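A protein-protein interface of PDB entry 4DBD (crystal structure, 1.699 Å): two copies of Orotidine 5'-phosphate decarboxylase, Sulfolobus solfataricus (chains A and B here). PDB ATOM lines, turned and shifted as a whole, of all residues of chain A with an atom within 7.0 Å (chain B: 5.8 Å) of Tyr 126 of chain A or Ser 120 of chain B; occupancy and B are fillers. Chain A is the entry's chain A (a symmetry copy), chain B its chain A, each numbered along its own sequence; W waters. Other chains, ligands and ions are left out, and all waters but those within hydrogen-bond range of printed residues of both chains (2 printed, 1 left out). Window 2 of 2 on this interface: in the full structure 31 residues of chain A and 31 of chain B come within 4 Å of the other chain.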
ATOM      1  N   SER A  86      21.850 -22.891   2.378  1.00  0.00           N
ATOM      2  CA  SER A  86      20.994 -23.188   1.231  1.00  0.00           C
ATOM      3  C   SER A  86      19.517 -23.226   1.597  1.00  0.00           C
ATOM      4  O   SER A  86      18.667 -22.839   0.792  1.00  0.00           O
ATOM      5  CB  SER A  86      21.347 -24.560   0.632  1.00  0.00           C
ATOM      6  OG  SER A  86      22.670 -24.590   0.142  1.00  0.00           O
ATOM      7  N   PHE A  87      19.199 -23.694   2.807  1.00  0.00           N
ATOM      8  CA  PHE A  87      17.800 -24.006   3.138  1.00  0.00           C
ATOM      9  C   PHE A  87      16.863 -22.797   3.103  1.00  0.00           C
ATOM     10  O   PHE A  87      15.637 -22.951   2.991  1.00  0.00           O
ATOM     11  CB  PHE A  87      17.676 -24.777   4.469  1.00  0.00           C
ATOM     12  CG  PHE A  87      17.840 -23.923   5.702  1.00  0.00           C
ATOM     13  CD1 PHE A  87      16.767 -23.209   6.220  1.00  0.00           C
ATOM     14  CD2 PHE A  87      19.054 -23.872   6.365  1.00  0.00           C
ATOM     15  CE1 PHE A  87      16.919 -22.428   7.364  1.00  0.00           C
ATOM     16  CE2 PHE A  87      19.210 -23.102   7.502  1.00  0.00           C
ATOM     17  CZ  PHE A  87      18.144 -22.379   8.003  1.00  0.00           C
ATOM     18  N   ILE A  88      17.435 -21.599   3.156  1.00  0.00           N
ATOM     19  CA  ILE A  88      16.616 -20.377   3.104  1.00  0.00           C
ATOM     20  C   ILE A  88      15.998 -20.111   1.734  1.00  0.00           C
ATOM     21  O   ILE A  88      15.049 -19.334   1.617  1.00  0.00           O
ATOM     22  CB  ILE A  88      17.397 -19.138   3.553  1.00  0.00           C
ATOM     23  CG1 ILE A  88      18.570 -18.873   2.619  1.00  0.00           C
ATOM     24  CG2 ILE A  88      17.889 -19.313   4.996  1.00  0.00           C
ATOM     25  CD1 ILE A  88      19.492 -17.787   3.151  1.00  0.00           C
ATOM     26  N   GLY A  89      16.552 -20.731   0.698  1.00  0.00           N
ATOM     27  CA  GLY A  89      15.943 -20.656  -0.614  1.00  0.00           C
ATOM     28  C   GLY A  89      16.389 -19.464  -1.434  1.00  0.00           C
ATOM     29  O   GLY A  89      17.224 -18.650  -1.006  1.00  0.00           O
ATOM     30  N   VAL A  90      15.811 -19.339  -2.624  1.00  0.00           N
ATOM     31  CA  VAL A  90      16.340 -18.409  -3.615  1.00  0.00           C
ATOM     32  C   VAL A  90      15.603 -17.064  -3.646  1.00  0.00           C
ATOM     33  O   VAL A  90      16.163 -16.031  -3.299  1.00  0.00           O
ATOM     34  CB  VAL A  90      16.343 -19.066  -5.020  1.00  0.00           C
ATOM     35  CG1 VAL A  90      16.789 -18.068  -6.106  1.00  0.00           C
ATOM     36  CG2 VAL A  90      17.224 -20.321  -5.016  1.00  0.00           C
ATOM     37  N   LEU A 122      16.553 -35.044   4.948  1.00  0.00           N
ATOM     38  CA  LEU A 122      15.304 -35.147   4.193  1.00  0.00           C
ATOM     39  C   LEU A 122      15.160 -34.177   3.025  1.00  0.00           C
ATOM     40  O   LEU A 122      14.317 -34.374   2.151  1.00  0.00           O
ATOM     41  CB  LEU A 122      14.110 -34.993   5.135  1.00  0.00           C
ATOM     42  CG  LEU A 122      14.040 -36.041   6.244  1.00  0.00           C
ATOM     43  CD1 LEU A 122      12.767 -35.878   7.065  1.00  0.00           C
ATOM     44  CD2 LEU A 122      14.132 -37.439   5.646  1.00  0.00           C
ATOM     45  N   PHE A 123      15.966 -33.126   3.005  1.00  0.00           N
ATOM     46  CA  PHE A 123      15.757 -32.076   2.015  1.00  0.00           C
ATOM     47  C   PHE A 123      16.964 -31.893   1.116  1.00  0.00           C
ATOM     48  O   PHE A 123      17.237 -30.793   0.627  1.00  0.00           O
ATOM     49  CB  PHE A 123      15.393 -30.779   2.727  1.00  0.00           C
ATOM     50  CG  PHE A 123      14.564 -30.999   3.956  1.00  0.00           C
ATOM     51  CD1 PHE A 123      13.428 -31.795   3.908  1.00  0.00           C
ATOM     52  CD2 PHE A 123      14.950 -30.461   5.170  1.00  0.00           C
ATOM     53  CE1 PHE A 123      12.666 -32.019   5.044  1.00  0.00           C
ATOM     54  CE2 PHE A 123      14.193 -30.680   6.308  1.00  0.00           C
ATOM     55  CZ  PHE A 123      13.052 -31.466   6.243  1.00  0.00           C
ATOM     56  N   ALA A 124      17.666 -32.996   0.883  1.00  0.00           N
ATOM     57  CA  ALA A 124      18.833 -33.002   0.012  1.00  0.00           C
ATOM     58  C   ALA A 124      18.479 -32.516  -1.391  1.00  0.00           C
ATOM     59  O   ALA A 124      19.246 -31.766  -1.994  1.00  0.00           O
ATOM     60  CB  ALA A 124      19.437 -34.392  -0.044  1.00  0.00           C
ATOM     61  N   ASP A 125      17.326 -32.951  -1.900  1.00  0.00           N
ATOM     62  CA  ASP A 125      16.883 -32.613  -3.253  1.00  0.00           C
ATOM     63  C   ASP A 125      16.592 -31.131  -3.361  1.00  0.00           C
ATOM     64  O   ASP A 125      17.030 -30.471  -4.305  1.00  0.00           O
ATOM     65  CB  ASP A 125      15.633 -33.424  -3.646  1.00  0.00           C
ATOM     66  CG  ASP A 125      15.941 -34.888  -3.904  1.00  0.00           C
ATOM     67  OD1 ASP A 125      16.948 -35.169  -4.586  1.00  0.00           O
ATOM     68  OD2 ASP A 125      15.176 -35.760  -3.424  1.00  0.00           O
ATOM     69  N   TYR A 126      15.850 -30.603  -2.396  1.00  0.00           N
ATOM     70  CA  TYR A 126      15.601 -29.166  -2.339  1.00  0.00           C
ATOM     71  C   TYR A 126      16.910 -28.369  -2.277  1.00  0.00           C
ATOM     72  O   TYR A 126      17.119 -27.428  -3.033  1.00  0.00           O
ATOM     73  CB  TYR A 126      14.749 -28.822  -1.124  1.00  0.00           C
ATOM     74  CG  TYR A 126      14.451 -27.341  -1.033  1.00  0.00           C
ATOM     75  CD1 TYR A 126      13.679 -26.713  -2.005  1.00  0.00           C
ATOM     76  CD2 TYR A 126      14.949 -26.568   0.014  1.00  0.00           C
ATOM     77  CE1 TYR A 126      13.398 -25.364  -1.940  1.00  0.00           C
ATOM     78  CE2 TYR A 126      14.673 -25.212   0.090  1.00  0.00           C
ATOM     79  CZ  TYR A 126      13.898 -24.616  -0.890  1.00  0.00           C
ATOM     80  OH  TYR A 126      13.623 -23.273  -0.823  1.00  0.00           O
ATOM     81  N   ILE A 127      17.788 -28.747  -1.357  1.00  0.00           N
ATOM     82  CA  ILE A 127      19.038 -28.021  -1.189  1.00  0.00           C
ATOM     83  C   ILE A 127      19.890 -28.099  -2.462  1.00  0.00           C
ATOM     84  O   ILE A 127      20.443 -27.101  -2.904  1.00  0.00           O
ATOM     85  CB  ILE A 127      19.798 -28.496   0.088  1.00  0.00           C
ATOM     86  CG1 ILE A 127      19.219 -27.760   1.314  1.00  0.00           C
ATOM     87  CG2 ILE A 127      21.278 -28.201  -0.034  1.00  0.00           C
ATOM     88  CD1 ILE A 127      19.491 -28.436   2.648  1.00  0.00           C
ATOM     89  N   LYS A 128      19.979 -29.278  -3.067  1.00  0.00           N
ATOM     90  CA  LYS A 128      20.703 -29.405  -4.334  1.00  0.00           C
ATOM     91  C   LYS A 128      20.126 -28.504  -5.416  1.00  0.00           C
ATOM     92  O   LYS A 128      20.873 -27.872  -6.169  1.00  0.00           O
ATOM     93  CB  LYS A 128      20.749 -30.870  -4.792  1.00  0.00           C
ATOM     94  CG  LYS A 128      21.684 -31.706  -3.944  1.00  0.00           C
ATOM     95  CD  LYS A 128      21.795 -33.151  -4.438  1.00  0.00           C
ATOM     96  CE  LYS A 128      22.720 -33.956  -3.531  1.00  0.00           C
ATOM     97  NZ  LYS A 128      23.054 -35.290  -4.118  1.00  0.00           N
ATOM     98  N   ASN A 129      18.803 -28.433  -5.494  1.00  0.00           N
ATOM     99  CA  ASN A 129      18.159 -27.517  -6.431  1.00  0.00           C
ATOM    100  C   ASN A 129      18.493 -26.055  -6.168  1.00  0.00           C
ATOM    101  O   ASN A 129      18.755 -25.289  -7.091  1.00  0.00           O
ATOM    102  CB  ASN A 129      16.647 -27.714  -6.425  1.00  0.00           C
ATOM    103  CG  ASN A 129      16.245 -28.987  -7.106  1.00  0.00           C
ATOM    104  OD1 ASN A 129      17.041 -29.573  -7.843  1.00  0.00           O
ATOM    105  ND2 ASN A 129      15.016 -29.434  -6.864  1.00  0.00           N
ATOM    106  N   VAL A 130      18.457 -25.657  -4.905  1.00  0.00           N
ATOM    107  CA  VAL A 130      18.880 -24.307  -4.552  1.00  0.00           C
ATOM    108  C   VAL A 130      20.304 -24.067  -5.038  1.00  0.00           C
ATOM    109  O   VAL A 130      20.609 -23.025  -5.631  1.00  0.00           O
ATOM    110  CB  VAL A 130      18.769 -24.065  -3.041  1.00  0.00           C
ATOM    111  CG1 VAL A 130      19.404 -22.751  -2.678  1.00  0.00           C
ATOM    112  CG2 VAL A 130      17.308 -24.095  -2.614  1.00  0.00           C
ATOM    113  N   ILE A 131      21.189 -25.028  -4.785  1.00  0.00           N
ATOM    114  CA  ILE A 131      22.583 -24.863  -5.190  1.00  0.00           C
ATOM    115  C   ILE A 131      22.703 -24.760  -6.708  1.00  0.00           C
ATOM    116  O   ILE A 131      23.465 -23.949  -7.229  1.00  0.00           O
ATOM    117  CB  ILE A 131      23.475 -26.001  -4.635  1.00  0.00           C
ATOM    118  CG1 ILE A 131      23.555 -25.882  -3.109  1.00  0.00           C
ATOM    119  CG2 ILE A 131      24.856 -25.954  -5.252  1.00  0.00           C
ATOM    120  CD1 ILE A 131      24.111 -27.125  -2.409  1.00  0.00           C
ATOM    121  N   ARG A 132      21.939 -25.579  -7.419  1.00  0.00           N
ATOM    122  CA  ARG A 132      21.926 -25.506  -8.883  1.00  0.00           C
ATOM    123  C   ARG A 132      21.459 -24.157  -9.442  1.00  0.00           C
ATOM    124  O   ARG A 132      22.044 -23.647 -10.395  1.00  0.00           O
ATOM    125  CB  ARG A 132      21.089 -26.644  -9.461  1.00  0.00           C
ATOM    126  CG  ARG A 132      21.706 -27.999  -9.244  1.00  0.00           C
ATOM    127  CD  ARG A 132      20.689 -29.094  -9.503  1.00  0.00           C
ATOM    128  NE  ARG A 132      21.272 -30.414  -9.319  1.00  0.00           N
ATOM    129  CZ  ARG A 132      20.668 -31.415  -8.687  1.00  0.00           C
ATOM    130  NH1 ARG A 132      19.448 -31.251  -8.188  1.00  0.00           N
ATOM    131  NH2 ARG A 132      21.282 -32.580  -8.563  1.00  0.00           N
ATOM    132  N   GLU B 117       9.418 -15.186  -0.754  1.00  0.00           N
ATOM    133  CA  GLU B 117       8.819 -16.197  -1.617  1.00  0.00           C
ATOM    134  C   GLU B 117       9.649 -17.471  -1.690  1.00  0.00           C
ATOM    135  O   GLU B 117       9.099 -18.561  -1.871  1.00  0.00           O
ATOM    136  CB  GLU B 117       8.589 -15.639  -3.027  1.00  0.00           C
ATOM    137  CG  GLU B 117       7.321 -14.832  -3.165  1.00  0.00           C
ATOM    138  CD  GLU B 117       7.181 -14.207  -4.540  1.00  0.00           C
ATOM    139  OE1 GLU B 117       6.921 -12.990  -4.607  1.00  0.00           O
ATOM    140  OE2 GLU B 117       7.330 -14.933  -5.549  1.00  0.00           O
ATOM    141  N   GLY B 118      10.965 -17.328  -1.533  1.00  0.00           N
ATOM    142  CA  GLY B 118      11.880 -18.442  -1.665  1.00  0.00           C
ATOM    143  C   GLY B 118      11.844 -19.410  -0.495  1.00  0.00           C
ATOM    144  O   GLY B 118      12.405 -20.500  -0.574  1.00  0.00           O
ATOM    145  N   TRP B 119      11.183 -19.023   0.592  1.00  0.00           N
ATOM    146  CA  TRP B 119      11.066 -19.921   1.740  1.00  0.00           C
ATOM    147  C   TRP B 119      10.199 -21.123   1.404  1.00  0.00           C
ATOM    148  O   TRP B 119       9.017 -20.974   1.076  1.00  0.00           O
ATOM    149  CB  TRP B 119      10.480 -19.202   2.959  1.00  0.00           C
ATOM    150  CG  TRP B 119      10.361 -20.105   4.159  1.00  0.00           C
ATOM    151  CD1 TRP B 119       9.249 -20.769   4.583  1.00  0.00           C
ATOM    152  CD2 TRP B 119      11.407 -20.453   5.074  1.00  0.00           C
ATOM    153  NE1 TRP B 119       9.532 -21.500   5.712  1.00  0.00           N
ATOM    154  CE2 TRP B 119      10.855 -21.322   6.034  1.00  0.00           C
ATOM    155  CE3 TRP B 119      12.759 -20.102   5.174  1.00  0.00           C
ATOM    156  CZ2 TRP B 119      11.608 -21.854   7.086  1.00  0.00           C
ATOM    157  CZ3 TRP B 119      13.501 -20.617   6.225  1.00  0.00           C
ATOM    158  CH2 TRP B 119      12.925 -21.486   7.164  1.00  0.00           C
ATOM    159  N   SER B 120      10.780 -22.314   1.512  1.00  0.00           N
ATOM    160  CA  SER B 120      10.068 -23.542   1.187  1.00  0.00           C
ATOM    161  C   SER B 120       9.049 -23.941   2.249  1.00  0.00           C
ATOM    162  O   SER B 120       9.318 -23.903   3.453  1.00  0.00           O
ATOM    163  CB  SER B 120      11.043 -24.698   0.950  1.00  0.00           C
ATOM    164  OG  SER B 120      10.334 -25.867   0.590  1.00  0.00           O
ATOM    165  N   THR B 121       7.878 -24.333   1.771  1.00  0.00           N
ATOM    166  CA  THR B 121       6.785 -24.779   2.610  1.00  0.00           C
ATOM    167  C   THR B 121       6.941 -26.269   2.888  1.00  0.00           C
ATOM    168  O   THR B 121       6.248 -26.831   3.737  1.00  0.00           O
ATOM    169  CB  THR B 121       5.445 -24.550   1.876  1.00  0.00           C
ATOM    170  OG1 THR B 121       4.404 -24.277   2.819  1.00  0.00           O
ATOM    171  CG2 THR B 121       5.077 -25.772   1.023  1.00  0.00           C
ATOM    172  N   LEU B 122       7.865 -26.903   2.175  1.00  0.00           N
ATOM    173  CA  LEU B 122       7.915 -28.363   2.095  1.00  0.00           C
ATOM    174  C   LEU B 122       8.252 -29.081   3.397  1.00  0.00           C
ATOM    175  O   LEU B 122       8.023 -30.283   3.524  1.00  0.00           O
ATOM    176  CB  LEU B 122       8.898 -28.793   1.005  1.00  0.00           C
ATOM    177  CG  LEU B 122       8.551 -28.288  -0.395  1.00  0.00           C
ATOM    178  CD1 LEU B 122       9.518 -28.851  -1.428  1.00  0.00           C
ATOM    179  CD2 LEU B 122       7.111 -28.649  -0.735  1.00  0.00           C
ATOM    180  N   PHE B 123       8.803 -28.361   4.363  1.00  0.00           N
ATOM    181  CA  PHE B 123       9.309 -29.026   5.559  1.00  0.00           C
ATOM    182  C   PHE B 123       8.615 -28.539   6.816  1.00  0.00           C
ATOM    183  O   PHE B 123       9.200 -28.519   7.903  1.00  0.00           O
ATOM    184  CB  PHE B 123      10.816 -28.830   5.644  1.00  0.00           C
ATOM    185  CG  PHE B 123      11.482 -28.822   4.302  1.00  0.00           C
ATOM    186  CD1 PHE B 123      11.233 -29.834   3.384  1.00  0.00           C
ATOM    187  CD2 PHE B 123      12.310 -27.777   3.933  1.00  0.00           C
ATOM    188  CE1 PHE B 123      11.831 -29.825   2.133  1.00  0.00           C
ATOM    189  CE2 PHE B 123      12.910 -27.763   2.686  1.00  0.00           C
ATOM    190  CZ  PHE B 123      12.663 -28.787   1.784  1.00  0.00           C
ATOM    191  N   ALA B 124       7.349 -28.171   6.656  1.00  0.00           N
ATOM    192  CA  ALA B 124       6.529 -27.712   7.769  1.00  0.00           C
ATOM    193  C   ALA B 124       6.445 -28.769   8.866  1.00  0.00           C
ATOM    194  O   ALA B 124       6.510 -28.435  10.049  1.00  0.00           O
ATOM    195  CB  ALA B 124       5.141 -27.345   7.278  1.00  0.00           C
HETATM  196  O   HOH W   1      10.954 -22.708  -2.233  1.00  0.00           O
HETATM  197  O   HOH W   2      13.991 -21.580  -3.320  1.00  0.00           O
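Ile 88 of chain A touches Gly 118 of chain B. Gly 89 of chain A touches Gly 118 of chain B. Phe 123 of chain A touches Phe 123 of chain B (CD1 to CD1, 3.0 Å). CB of Ser 120 of chain B touches CZ of Tyr 126 of chain A (3.4 Å). Tyr 126 of chain A touches Phe 123 of chain B.
Of the 8 printed residues of chain B, 3 touch a printed residue of chain A. Printed residues of chain B that touch a printed residue of chain A: Gly 118, Ser 120 and Phe 123. Hydrophobic or aromatic side chains of chain A that line the printed part of chain B: Phe 123 and Tyr 126. Among the printed residues, 6 pairs touch across the chains. Among the printed residues, no Asp or Glu carboxylate lies within 4 Å of a Lys or Arg side-chain nitrogen of the other chain.
The backbone carbonyl oxygen of Gly 118 of chain B lies within hydrogen-bond range of the side-chain hydroxyl of Tyr 126 of chain A, 3.0 Å away.
Phe 123 of chain A touches its own counterpart, Phe 123 of chain B. Positions printed for both chains: 122, 123 and 124. Of the 6 pairs that touch across the chains among the printed residues, 1 has its exchanged pair printed and touching as well.
Water W2 lies within hydrogen-bond range of N of Val 90 of chain A (3.0 Å), OH of Tyr 126 of chain A (3.0 Å) and O of Gly 118 of chain B (3.3 Å). Water W1 lies within hydrogen-bond range of OH of Tyr 126 of chain A (3.1 Å) and O of Gly 118 of chain B (3.1 Å).
The side-chain hydroxyl (OG) of Ser 120 of chain B is in hydrogen-bond range of the backbone NH (N) of Leu 122 of chain B, 3.1 Å away.
Of chain A, only Tyr 126 (3.4 Å) comes within 4 Å of Ser 120 of chain B. Of the printed residues of chain A, Gly 118 of chain B touches Ile 88 (3.6 Å), Gly 89 (3.5 Å) and Tyr 126 (3.0 Å). Printed residues of chain B within 4 Å of Ile 88 of chain A: Gly 118 (3.6 Å). Of the printed residues of chain B, Phe 123 of chain A touches Phe 123 (3.0 Å). Of the printed residues of chain A, Phe 123 of chain B touches Phe 123 (3.0 Å) and Tyr 126 (3.6 Å). Lys 128 of chain A touches none of the printed residues of chain B. Ser 86 of chain A touches none of the printed residues of chain B. The nearest residue of chain B that does not touch Tyr 126 of chain A is Trp 119 of chain B (4.6 Å). The nearest printed residue of chain A that does not touch Ser 120 of chain B is Phe 87 of chain A (5.1 Å).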
